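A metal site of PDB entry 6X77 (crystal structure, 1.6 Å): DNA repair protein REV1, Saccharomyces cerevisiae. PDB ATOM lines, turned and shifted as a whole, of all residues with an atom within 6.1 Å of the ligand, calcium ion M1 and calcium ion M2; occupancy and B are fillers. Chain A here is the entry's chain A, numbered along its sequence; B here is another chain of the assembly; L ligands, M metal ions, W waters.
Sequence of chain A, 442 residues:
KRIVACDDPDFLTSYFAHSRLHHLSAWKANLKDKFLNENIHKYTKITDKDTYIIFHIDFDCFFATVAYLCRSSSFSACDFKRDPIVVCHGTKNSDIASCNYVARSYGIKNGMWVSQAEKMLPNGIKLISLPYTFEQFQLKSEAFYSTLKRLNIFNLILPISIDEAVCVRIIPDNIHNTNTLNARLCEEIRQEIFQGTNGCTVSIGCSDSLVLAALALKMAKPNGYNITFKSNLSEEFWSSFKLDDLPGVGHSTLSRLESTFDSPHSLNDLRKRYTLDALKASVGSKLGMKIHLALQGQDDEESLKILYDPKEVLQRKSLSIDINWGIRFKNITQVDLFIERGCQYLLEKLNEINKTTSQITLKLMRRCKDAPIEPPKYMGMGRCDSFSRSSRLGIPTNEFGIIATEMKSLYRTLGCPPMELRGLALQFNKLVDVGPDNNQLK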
ATOM      1  N   ARG A  20     -11.230  11.167  12.683  1.00  0.00           N
ATOM      2  CA  ARG A  20     -11.083  12.107  13.797  1.00  0.00           C
ATOM      3  C   ARG A  20     -12.409  12.788  14.136  1.00  0.00           C
ATOM      4  O   ARG A  20     -12.642  13.123  15.317  1.00  0.00           O
ATOM      5  CB  ARG A  20      -9.973  13.104  13.489  1.00  0.00           C
ATOM      6  CG  ARG A  20     -10.448  14.461  13.034  1.00  0.00           C
ATOM      7  CD  ARG A  20     -10.701  14.570  11.508  1.00  0.00           C
ATOM      8  NE  ARG A  20     -10.929  15.960  11.121  1.00  0.00           N
ATOM      9  CZ  ARG A  20     -11.241  16.384   9.901  1.00  0.00           C
ATOM     10  NH1 ARG A  20     -11.453  15.532   8.881  1.00  0.00           N
ATOM     11  NH2 ARG A  20     -11.342  17.710   9.702  1.00  0.00           N
ATOM     12  N   LEU A  21     -13.285  12.974  13.151  1.00  0.00           N
ATOM     13  CA  LEU A  21     -14.582  13.572  13.455  1.00  0.00           C
ATOM     14  C   LEU A  21     -15.424  12.628  14.313  1.00  0.00           C
ATOM     15  O   LEU A  21     -16.080  13.074  15.264  1.00  0.00           O
ATOM     16  CB  LEU A  21     -15.306  13.977  12.174  1.00  0.00           C
ATOM     17  CG  LEU A  21     -14.568  15.102  11.404  1.00  0.00           C
ATOM     18  CD1 LEU A  21     -15.230  15.404  10.114  1.00  0.00           C
ATOM     19  CD2 LEU A  21     -14.406  16.383  12.199  1.00  0.00           C
ATOM     20  N   LEU A  24     -13.897  13.043  17.820  1.00  0.00           N
ATOM     21  CA  LEU A  24     -14.344  14.294  18.429  1.00  0.00           C
ATOM     22  C   LEU A  24     -15.732  14.151  19.034  1.00  0.00           C
ATOM     23  O   LEU A  24     -15.933  14.481  20.190  1.00  0.00           O
ATOM     24  CB  LEU A  24     -14.352  15.426  17.411  1.00  0.00           C
ATOM     25  CG  LEU A  24     -12.990  15.996  17.103  1.00  0.00           C
ATOM     26  CD1 LEU A  24     -13.208  17.120  16.058  1.00  0.00           C
ATOM     27  CD2 LEU A  24     -12.253  16.565  18.277  1.00  0.00           C
ATOM     28  N   ASP A  58      -8.714  26.566  26.316  1.00  0.00           N
ATOM     29  CA  ASP A  58      -8.659  25.742  25.100  1.00  0.00           C
ATOM     30  C   ASP A  58      -7.222  25.504  24.663  1.00  0.00           C
ATOM     31  O   ASP A  58      -6.404  26.427  24.645  1.00  0.00           O
ATOM     32  CB  ASP A  58      -9.491  26.445  24.017  1.00  0.00           C
ATOM     33  CG  ASP A  58      -9.266  25.865  22.637  1.00  0.00           C
ATOM     34  OD1 ASP A  58      -9.985  24.900  22.297  1.00  0.00           O
ATOM     35  OD2 ASP A  58      -8.330  26.347  21.954  1.00  0.00           O
ATOM     36  N   PHE A  59      -6.916  24.247  24.314  1.00  0.00           N
ATOM     37  CA  PHE A  59      -5.569  23.933  23.827  1.00  0.00           C
ATOM     38  C   PHE A  59      -5.299  24.653  22.499  1.00  0.00           C
ATOM     39  O   PHE A  59      -6.134  24.600  21.589  1.00  0.00           O
ATOM     40  CB  PHE A  59      -5.404  22.432  23.530  1.00  0.00           C
ATOM     41  CG  PHE A  59      -5.198  21.547  24.709  1.00  0.00           C
ATOM     42  CD1 PHE A  59      -6.257  21.165  25.485  1.00  0.00           C
ATOM     43  CD2 PHE A  59      -3.969  20.964  24.910  1.00  0.00           C
ATOM     44  CE1 PHE A  59      -6.089  20.219  26.527  1.00  0.00           C
ATOM     45  CE2 PHE A  59      -3.766  20.005  25.915  1.00  0.00           C
ATOM     46  CZ  PHE A  59      -4.840  19.666  26.738  1.00  0.00           C
ATOM     47  N   ASP A  60      -4.099  25.262  22.370  1.00  0.00           N
ATOM     48  CA  ASP A  60      -3.641  25.775  21.085  1.00  0.00           C
ATOM     49  C   ASP A  60      -3.246  24.695  20.069  1.00  0.00           C
ATOM     50  O   ASP A  60      -2.430  23.805  20.353  1.00  0.00           O
ATOM     51  CB  ASP A  60      -2.362  26.627  21.270  1.00  0.00           C
ATOM     52  CG  ASP A  60      -2.583  27.749  22.252  1.00  0.00           C
ATOM     53  OD1 ASP A  60      -3.600  28.467  22.132  1.00  0.00           O
ATOM     54  OD2 ASP A  60      -1.736  27.868  23.155  1.00  0.00           O
ATOM     55  N   CYS A  61      -3.833  24.788  18.866  1.00  0.00           N
ATOM     56  CA  CYS A  61      -3.697  23.818  17.782  1.00  0.00           C
ATOM     57  C   CYS A  61      -3.530  22.395  18.316  1.00  0.00           C
ATOM     58  O   CYS A  61      -2.484  21.752  18.147  1.00  0.00           O
ATOM     59  CB  CYS A  61      -2.541  24.189  16.866  1.00  0.00           C
ATOM     60  SG  CYS A  61      -0.931  24.544  17.711  1.00  0.00           S
ATOM     61  N   PHE A  62      -4.594  21.897  18.946  1.00  0.00           N
ATOM     62  CA  PHE A  62      -4.502  20.730  19.822  1.00  0.00           C
ATOM     63  C   PHE A  62      -3.850  19.514  19.171  1.00  0.00           C
ATOM     64  O   PHE A  62      -2.873  18.984  19.698  1.00  0.00           O
ATOM     65  CB  PHE A  62      -5.906  20.398  20.334  1.00  0.00           C
ATOM     66  CG  PHE A  62      -5.982  19.202  21.245  1.00  0.00           C
ATOM     67  CD1 PHE A  62      -5.210  19.124  22.391  1.00  0.00           C
ATOM     68  CD2 PHE A  62      -6.887  18.173  20.977  1.00  0.00           C
ATOM     69  CE1 PHE A  62      -5.303  18.040  23.235  1.00  0.00           C
ATOM     70  CE2 PHE A  62      -7.012  17.087  21.852  1.00  0.00           C
ATOM     71  CZ  PHE A  62      -6.206  17.003  22.955  1.00  0.00           C
ATOM     72  N   PHE A  63      -4.445  18.996  18.089  1.00  0.00           N
ATOM     73  CA  PHE A  63      -3.875  17.773  17.514  1.00  0.00           C
ATOM     74  C   PHE A  63      -2.434  18.029  17.073  1.00  0.00           C
ATOM     75  O   PHE A  63      -1.592  17.151  17.209  1.00  0.00           O
ATOM     76  CB  PHE A  63      -4.637  17.237  16.299  1.00  0.00           C
ATOM     77  CG  PHE A  63      -5.943  16.543  16.602  1.00  0.00           C
ATOM     78  CD1 PHE A  63      -6.489  16.525  17.876  1.00  0.00           C
ATOM     79  CD2 PHE A  63      -6.626  15.888  15.577  1.00  0.00           C
ATOM     80  CE1 PHE A  63      -7.706  15.944  18.121  1.00  0.00           C
ATOM     81  CE2 PHE A  63      -7.856  15.281  15.819  1.00  0.00           C
ATOM     82  CZ  PHE A  63      -8.380  15.293  17.086  1.00  0.00           C
ATOM     83  N   ALA A  64      -2.168  19.196  16.465  1.00  0.00           N
ATOM     84  CA  ALA A  64      -0.810  19.492  15.986  1.00  0.00           C
ATOM     85  C   ALA A  64       0.171  19.487  17.151  1.00  0.00           C
ATOM     86  O   ALA A  64       1.219  18.831  17.075  1.00  0.00           O
ATOM     87  CB  ALA A  64      -0.785  20.811  15.209  1.00  0.00           C
ATOM     88  N   ASP A  95      -8.064  16.026   4.800  1.00  0.00           N
ATOM     89  CA  ASP A  95      -8.268  17.139   5.714  1.00  0.00           C
ATOM     90  C   ASP A  95      -7.054  17.372   6.618  1.00  0.00           C
ATOM     91  O   ASP A  95      -6.491  16.450   7.205  1.00  0.00           O
ATOM     92  CB  ASP A  95      -9.496  16.922   6.587  1.00  0.00           C
ATOM     93  CG  ASP A  95     -10.802  17.256   5.897  1.00  0.00           C
ATOM     94  OD1 ASP A  95     -10.898  17.347   4.653  1.00  0.00           O
ATOM     95  OD2 ASP A  95     -11.782  17.374   6.643  1.00  0.00           O
ATOM     96  N   ILE A  96      -6.689  18.634   6.744  1.00  0.00           N
ATOM     97  CA  ILE A  96      -5.836  19.114   7.823  1.00  0.00           C
ATOM     98  C   ILE A  96      -6.712  19.239   9.074  1.00  0.00           C
ATOM     99  O   ILE A  96      -7.470  20.205   9.250  1.00  0.00           O
ATOM    100  CB  ILE A  96      -5.164  20.443   7.446  1.00  0.00           C
ATOM    101  CG1 ILE A  96      -4.162  20.192   6.305  1.00  0.00           C
ATOM    102  CG2 ILE A  96      -4.488  21.025   8.652  1.00  0.00           C
ATOM    103  CD1 ILE A  96      -3.813  21.480   5.521  1.00  0.00           C
ATOM    104  N   ALA A  97      -6.601  18.251   9.972  1.00  0.00           N
ATOM    105  CA  ALA A  97      -7.386  18.291  11.207  1.00  0.00           C
ATOM    106  C   ALA A  97      -6.960  19.449  12.089  1.00  0.00           C
ATOM    107  O   ALA A  97      -7.828  20.101  12.696  1.00  0.00           O
ATOM    108  CB  ALA A  97      -7.282  16.961  11.977  1.00  0.00           C
ATOM    109  N   SER A  98      -5.639  19.714  12.174  1.00  0.00           N
ATOM    110  CA  SER A  98      -5.049  20.788  12.974  1.00  0.00           C
ATOM    111  C   SER A  98      -3.744  21.220  12.314  1.00  0.00           C
ATOM    112  O   SER A  98      -3.012  20.375  11.768  1.00  0.00           O
ATOM    113  CB  SER A  98      -4.813  20.366  14.436  1.00  0.00           C
ATOM    114  OG  SER A  98      -4.372  21.432  15.286  1.00  0.00           O
ATOM    115  N   CYS A  99      -3.464  22.517  12.379  1.00  0.00           N
ATOM    116  CA  CYS A  99      -2.209  23.091  11.901  1.00  0.00           C
ATOM    117  C   CYS A  99      -1.669  24.041  12.950  1.00  0.00           C
ATOM    118  O   CYS A  99      -2.435  24.679  13.710  1.00  0.00           O
ATOM    119  CB  CYS A  99      -2.406  23.792  10.545  1.00  0.00           C
ATOM    120  SG  CYS A  99      -3.640  25.113  10.554  1.00  0.00           S
ATOM    121  N   TYR A 101       0.788  27.305  14.404  1.00  0.00           N
ATOM    122  CA  TYR A 101       0.603  28.723  14.064  1.00  0.00           C
ATOM    123  C   TYR A 101       1.608  29.179  13.028  1.00  0.00           C
ATOM    124  O   TYR A 101       1.293  30.110  12.287  1.00  0.00           O
ATOM    125  CB  TYR A 101       0.624  29.581  15.339  1.00  0.00           C
ATOM    126  CG  TYR A 101      -0.725  29.515  16.011  1.00  0.00           C
ATOM    127  CD1 TYR A 101      -1.178  28.340  16.629  1.00  0.00           C
ATOM    128  CD2 TYR A 101      -1.589  30.592  15.981  1.00  0.00           C
ATOM    129  CE1 TYR A 101      -2.448  28.278  17.184  1.00  0.00           C
ATOM    130  CE2 TYR A 101      -2.839  30.534  16.544  1.00  0.00           C
ATOM    131  CZ  TYR A 101      -3.276  29.385  17.148  1.00  0.00           C
ATOM    132  OH  TYR A 101      -4.529  29.360  17.724  1.00  0.00           O
ATOM    133  N   ARG A 104      -0.345  28.587   9.976  1.00  0.00           N
ATOM    134  CA  ARG A 104      -1.407  29.578   9.852  1.00  0.00           C
ATOM    135  C   ARG A 104      -0.893  30.948   9.415  1.00  0.00           C
ATOM    136  O   ARG A 104      -1.671  31.744   8.874  1.00  0.00           O
ATOM    137  CB  ARG A 104      -2.143  29.718  11.174  1.00  0.00           C
ATOM    138  CG  ARG A 104      -2.841  28.432  11.579  1.00  0.00           C
ATOM    139  CD  ARG A 104      -3.619  28.579  12.890  1.00  0.00           C
ATOM    140  NE  ARG A 104      -3.972  27.245  13.396  1.00  0.00           N
ATOM    141  CZ  ARG A 104      -4.860  27.002  14.347  1.00  0.00           C
ATOM    142  NH1 ARG A 104      -5.530  27.995  14.927  1.00  0.00           N
ATOM    143  NH2 ARG A 104      -5.081  25.730  14.699  1.00  0.00           N
ATOM    144  N   ASN A 110      -7.382  24.964   9.745  1.00  0.00           N
ATOM    145  CA  ASN A 110      -8.004  23.654  10.008  1.00  0.00           C
ATOM    146  C   ASN A 110      -9.135  23.412   9.021  1.00  0.00           C
ATOM    147  O   ASN A 110      -9.912  24.325   8.703  1.00  0.00           O
ATOM    148  CB  ASN A 110      -8.567  23.589  11.430  1.00  0.00           C
ATOM    149  CG  ASN A 110      -7.489  23.592  12.503  1.00  0.00           C
ATOM    150  OD1 ASN A 110      -6.294  23.557  12.220  1.00  0.00           O
ATOM    151  ND2 ASN A 110      -7.921  23.654  13.761  1.00  0.00           N
ATOM    152  N   GLY A 111      -9.216  22.191   8.514  1.00  0.00           N
ATOM    153  CA  GLY A 111     -10.231  21.797   7.558  1.00  0.00           C
ATOM    154  C   GLY A 111      -9.816  21.911   6.108  1.00  0.00           C
ATOM    155  O   GLY A 111     -10.465  21.307   5.242  1.00  0.00           O
ATOM    156  N   TYR A 132      -2.076  11.137  13.033  1.00  0.00           N
ATOM    157  CA  TYR A 132      -2.885  11.218  14.220  1.00  0.00           C
ATOM    158  C   TYR A 132      -2.308  10.348  15.337  1.00  0.00           C
ATOM    159  O   TYR A 132      -1.800   9.255  15.093  1.00  0.00           O
ATOM    160  CB  TYR A 132      -4.297  10.755  13.909  1.00  0.00           C
ATOM    161  CG  TYR A 132      -5.076  11.619  12.917  1.00  0.00           C
ATOM    162  CD1 TYR A 132      -5.058  11.369  11.555  1.00  0.00           C
ATOM    163  CD2 TYR A 132      -5.851  12.675  13.364  1.00  0.00           C
ATOM    164  CE1 TYR A 132      -5.818  12.123  10.671  1.00  0.00           C
ATOM    165  CE2 TYR A 132      -6.562  13.478  12.465  1.00  0.00           C
ATOM    166  CZ  TYR A 132      -6.568  13.179  11.138  1.00  0.00           C
ATOM    167  OH  TYR A 132      -7.326  13.902  10.242  1.00  0.00           O
ATOM    168  N   SER A 161     -15.305  20.400  24.544  1.00  0.00           N
ATOM    169  CA  SER A 161     -14.780  19.356  23.669  1.00  0.00           C
ATOM    170  C   SER A 161     -13.533  18.775  24.339  1.00  0.00           C
ATOM    171  O   SER A 161     -13.174  19.129  25.464  1.00  0.00           O
ATOM    172  CB  SER A 161     -14.474  19.904  22.278  1.00  0.00           C
ATOM    173  OG  SER A 161     -13.277  20.667  22.355  1.00  0.00           O
ATOM    174  N   ILE A 162     -12.935  17.816  23.641  1.00  0.00           N
ATOM    175  CA  ILE A 162     -11.730  17.134  24.056  1.00  0.00           C
ATOM    176  C   ILE A 162     -10.701  18.149  24.572  1.00  0.00           C
ATOM    177  O   ILE A 162     -10.006  17.874  25.552  1.00  0.00           O
ATOM    178  CB  ILE A 162     -11.173  16.309  22.875  1.00  0.00           C
ATOM    179  CG1 ILE A 162     -10.006  15.429  23.369  1.00  0.00           C
ATOM    180  CG2 ILE A 162     -10.821  17.150  21.651  1.00  0.00           C
ATOM    181  CD1 ILE A 162     -10.455  14.374  24.249  1.00  0.00           C
ATOM    182  N   ASP A 163     -10.597  19.322  23.943  1.00  0.00           N
ATOM    183  CA  ASP A 163      -9.529  20.256  24.297  1.00  0.00           C
ATOM    184  C   ASP A 163     -10.028  21.589  24.846  1.00  0.00           C
ATOM    185  O   ASP A 163      -9.257  22.567  24.837  1.00  0.00           O
ATOM    186  CB  ASP A 163      -8.628  20.506  23.080  1.00  0.00           C
ATOM    187  CG  ASP A 163      -9.230  21.542  22.108  1.00  0.00           C
ATOM    188  OD1 ASP A 163     -10.469  21.560  21.971  1.00  0.00           O
ATOM    189  OD2 ASP A 163      -8.441  22.285  21.490  1.00  0.00           O
ATOM    190  N   GLU A 164     -11.249  21.649  25.372  1.00  0.00           N
ATOM    191  CA  GLU A 164     -11.850  22.958  25.614  1.00  0.00           C
ATOM    192  C   GLU A 164     -12.910  22.887  26.691  1.00  0.00           C
ATOM    193  O   GLU A 164     -13.767  21.988  26.670  1.00  0.00           O
ATOM    194  CB  GLU A 164     -12.449  23.492  24.321  1.00  0.00           C
ATOM    195  CG  GLU A 164     -13.025  24.861  24.360  1.00  0.00           C
ATOM    196  CD  GLU A 164     -13.503  25.326  22.986  1.00  0.00           C
ATOM    197  OE1 GLU A 164     -14.158  26.408  22.942  1.00  0.00           O
ATOM    198  OE2 GLU A 164     -13.277  24.582  21.964  1.00  0.00           O
ATOM    199  N   LYS A 218     -10.001  33.963  21.458  1.00  0.00           N
ATOM    200  CA  LYS A 218      -9.475  34.174  20.114  1.00  0.00           C
ATOM    201  C   LYS A 218      -8.356  35.212  20.113  1.00  0.00           C
ATOM    202  O   LYS A 218      -7.295  35.000  19.541  1.00  0.00           O
ATOM    203  CB  LYS A 218     -10.605  34.620  19.202  1.00  0.00           C
ATOM    204  CG  LYS A 218     -10.262  34.588  17.741  1.00  0.00           C
ATOM    205  CD  LYS A 218     -10.275  33.170  17.320  1.00  0.00           C
ATOM    206  CE  LYS A 218      -9.134  32.863  16.381  1.00  0.00           C
ATOM    207  NZ  LYS A 218      -8.687  34.035  15.535  1.00  0.00           N
ATOM    208  N   LYS A 221      -4.863  33.930  21.583  1.00  0.00           N
ATOM    209  CA  LYS A 221      -4.074  32.909  20.913  1.00  0.00           C
ATOM    210  C   LYS A 221      -2.979  33.502  20.023  1.00  0.00           C
ATOM    211  O   LYS A 221      -3.151  34.587  19.459  1.00  0.00           O
ATOM    212  CB  LYS A 221      -4.996  32.035  20.085  1.00  0.00           C
ATOM    213  CG  LYS A 221      -5.845  31.070  20.947  1.00  0.00           C
ATOM    214  CD  LYS A 221      -6.800  30.225  20.146  1.00  0.00           C
ATOM    215  CE  LYS A 221      -7.431  29.165  21.061  1.00  0.00           C
ATOM    216  NZ  LYS A 221      -6.447  28.072  21.375  1.00  0.00           N
ATOM    217  P    DG B  12     -18.138  24.453  20.002  1.00  0.00           P
ATOM    218  OP1  DG B  12     -19.212  24.105  20.830  1.00  0.00           O
ATOM    219  OP2  DG B  12     -17.625  25.779  20.017  1.00  0.00           O
ATOM    220  O5'  DG B  12     -17.003  23.398  20.349  1.00  0.00           O
ATOM    221  C5'  DG B  12     -15.682  23.553  19.869  1.00  0.00           C
ATOM    222  C4'  DG B  12     -15.199  22.264  19.222  1.00  0.00           C
ATOM    223  O4'  DG B  12     -15.905  22.049  18.030  1.00  0.00           O
ATOM    224  C3'  DG B  12     -13.747  22.328  18.796  1.00  0.00           C
ATOM    225  O3'  DG B  12     -12.916  21.856  19.831  1.00  0.00           O
ATOM    226  C2'  DG B  12     -13.702  21.439  17.569  1.00  0.00           C
ATOM    227  C1'  DG B  12     -15.153  21.102  17.306  1.00  0.00           C
ATOM    228  N9   DG B  12     -15.579  21.132  15.923  1.00  0.00           N
ATOM    229  C8   DG B  12     -15.305  22.049  14.942  1.00  0.00           C
ATOM    230  N7   DG B  12     -15.872  21.755  13.805  1.00  0.00           N
ATOM    231  C5   DG B  12     -16.531  20.564  14.046  1.00  0.00           C
ATOM    232  C6   DG B  12     -17.329  19.766  13.180  1.00  0.00           C
ATOM    233  O6   DG B  12     -17.550  19.914  11.998  1.00  0.00           O
ATOM    234  N1   DG B  12     -17.818  18.644  13.842  1.00  0.00           N
ATOM    235  C2   DG B  12     -17.595  18.343  15.156  1.00  0.00           C
ATOM    236  N2   DG B  12     -18.116  17.194  15.586  1.00  0.00           N
ATOM    237  N3   DG B  12     -16.850  19.072  15.965  1.00  0.00           N
ATOM    238  C4   DG B  12     -16.351  20.159  15.343  1.00  0.00           C
HETATM  239  N1  LIG L   1     -10.611  19.506  14.537  1.00  0.00           N
HETATM  240  C1  LIG L   1     -10.628  18.759  13.250  1.00  0.00           C
HETATM  241  N2  LIG L   1     -11.182  19.433  12.069  1.00  0.00           N
HETATM  242  C2  LIG L   1     -11.591  20.791  12.141  1.00  0.00           C
HETATM  243  C3  LIG L   1     -11.530  21.548  13.410  1.00  0.00           C
HETATM  244  C4  LIG L   1     -11.016  20.884  14.622  1.00  0.00           C
HETATM  245  O1  LIG L   1     -10.285  17.642  13.124  1.00  0.00           O
HETATM  246  N3  LIG L   1     -12.054  21.448  10.976  1.00  0.00           N
HETATM  247  C5  LIG L   1     -10.056  18.875  15.750  1.00  0.00           C
HETATM  248  C6  LIG L   1      -8.505  19.119  15.614  1.00  0.00           C
HETATM  249  C7  LIG L   1      -8.265  20.326  16.485  1.00  0.00           C
HETATM  250  C8  LIG L   1      -9.092  20.058  17.530  1.00  0.00           C
HETATM  251  O2  LIG L   1     -10.421  19.475  16.833  1.00  0.00           O
HETATM  252  O3  LIG L   1      -6.924  20.304  17.090  1.00  0.00           O
HETATM  253  C9  LIG L   1      -9.667  21.112  18.399  1.00  0.00           C
HETATM  254  O4  LIG L   1     -10.388  22.001  17.562  1.00  0.00           O
HETATM  255  P1  LIG L   1     -10.171  23.589  17.744  1.00  0.00           P
HETATM  256  O5  LIG L   1     -10.198  23.996  19.183  1.00  0.00           O
HETATM  257  O6  LIG L   1     -11.220  24.297  16.896  1.00  0.00           O
HETATM  258  O7  LIG L   1      -8.793  23.947  16.991  1.00  0.00           O
HETATM  259  P2  LIG L   1      -7.228  23.779  17.291  1.00  0.00           P
HETATM  260  O8  LIG L   1      -7.048  23.397  18.735  1.00  0.00           O
HETATM  261  O9  LIG L   1      -6.548  22.862  16.291  1.00  0.00           O
HETATM  262  O10 LIG L   1      -6.672  25.257  17.045  1.00  0.00           O
HETATM  263  P3  LIG L   1      -6.985  26.634  17.900  1.00  0.00           P
HETATM  264  O11 LIG L   1      -7.994  26.344  18.973  1.00  0.00           O
HETATM  265  O12 LIG L   1      -5.692  27.067  18.527  1.00  0.00           O
HETATM  266  O13 LIG L   1      -7.476  27.620  16.858  1.00  0.00           O
HETATM  267 CA    CA M   1      -8.193  24.397  20.483  1.00  0.00          CA
HETATM  268 CA    CA M   2     -11.446  23.451  20.900  1.00  0.00          CA
HETATM  269  O   HOH W   1      -8.935  26.967  14.736  1.00  0.00           O
HETATM  270  O   HOH W   2     -13.246  24.047  11.170  1.00  0.00           O
HETATM  271  O   HOH W   3     -13.132  20.049   8.604  1.00  0.00           O
HETATM  272  O   HOH W   4      -8.853  29.959  17.225  1.00  0.00           O
HETATM  273  O   HOH W   5     -10.567  24.718  14.157  1.00  0.00           O
HETATM  274  O   HOH W   6     -10.558  27.678  19.369  1.00  0.00           O
HETATM  275  O   HOH W   7     -13.994  25.016  16.570  1.00  0.00           O
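NZ of Lys 221 lies within salt-bridge range of O12 of the ligand (3.1 Å). O3 of the ligand is in hydrogen-bond range of N of Phe 62 (3.4 Å). An oxygen (O1) of the ligand lies within hydrogen-bond range of the guanidinium group of Arg 20, 2.7 Å away. The backbone NH (N) of Cys 61 lies within hydrogen-bond range of an oxygen (O12) of the ligand (3.0 Å). The side-chain amide nitrogen of Asn 110 lies within hydrogen-bond range of an oxygen (O9) of the ligand (3.0 Å). An oxygen (O3) of the ligand is in hydrogen-bond range of the backbone NH (N) of Phe 63 (3.0 Å). The guanidinium group (NH1) of Arg 104 is in salt-bridge range of an oxygen (O13) of the ligand. An oxygen (O12) of the ligand lies within hydrogen-bond range of the side-chain hydroxyl (OH) of Tyr 101, at 2.7 Å. An oxygen (O9) of the ligand is in hydrogen-bond range of the side-chain hydroxyl of Ser 98 (2.8 Å).
Calcium ion M1 is bound by O8 of the ligand (2.3 Å). O of Phe 59 is bound to calcium ion M1 (2.3 Å). OD2 of Asp 163 binds calcium ion M1 (2.4 Å). An oxygen (O5) of the ligand binds calcium ion M1. OD2 of Asp 58 is bound to calcium ion M1, 2.4 Å away. An oxygen (O11) of the ligand is bound to calcium ion M1 (2.5 Å). OD1 of Asp 58 is bound to calcium ion M1 (2.6 Å). Calcium ion M1 has seven donor atoms within binding distance.
Within 4 Å of calcium ion M1: Asp 58, Phe 59 and Asp 163.
A nitrogen (N1) of the ligand lies close to the backbone carbonyl oxygen (O) of Ala 97. CD1 of Leu 24 touches C5 of the ligand, at 3.6 Å. Asp 60 touches the ligand (CA to O12, 3.5 Å). Gly 111 touches the ligand (N to N3, 3.8 Å). 17 residues have an atom within 4 Å of the ligand: Arg 20, Leu 24, Asp 58, Phe 59, Asp 60, Cys 61, Phe 62, Phe 63, Ala 97, Ser 98, Tyr 101, Arg 104, Asn 110, Gly 111, Asp 163, Lys 221 and DG 12 of chain B. The nearest printed residue that does not touch the ligand is Glu 164 (4.2 Å).
Water W5 lies within hydrogen-bond range of an oxygen (O6) of the ligand and the side-chain amide nitrogen (ND2) of Asn 110. Water W3 lies within hydrogen-bond range of N3 of the ligand and NH2 of Arg 20.
The side-chain amino group (NZ) of Lys 221 sits close to the side-chain carboxylate (OD2) of Asp 58. The side-chain hydroxyl (OH) of Tyr 101 lies within hydrogen-bond range of the guanidinium group (NH1) of Arg 104 (3.3 Å). O3' of DG 12 of chain B lies close to OG of Ser 161, 2.8 Å away. N of Cys 99 lies within hydrogen-bond range of OD1 of Asn 110 (3.0 Å). The backbone NH (N) of Ala 64 lies within hydrogen-bond range of the side-chain hydroxyl (OG) of Ser 98 (3.4 Å). The side-chain amino group of Lys 221 lies close to the backbone carbonyl oxygen of Phe 59 (3.5 Å). The backbone carbonyl oxygen of Cys 61 lies close to the side-chain hydroxyl of Ser 98 (3.4 Å). NH1 of Arg 20 is in salt-bridge range of OD2 of Asp 95.
An oxygen (O5) of the ligand binds calcium ion M2. OD1 of Asp 163 is bound to calcium ion M2 (2.4 Å). OE2 of Glu 164 is bound to calcium ion M2. O3' of DG 12 of chain B binds calcium ion M2 (2.4 Å). OD1 of Asp 58 binds calcium ion M2 (2.5 Å). Calcium ion M2 has five donor atoms within binding distance.
OG of Ser 161 touches calcium ion M2 (3.6 Å). Five residues have an atom within 4 Å of calcium ion M2: Asp 58, Ser 161, Asp 163, Glu 164 and DG 12 of chain B.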
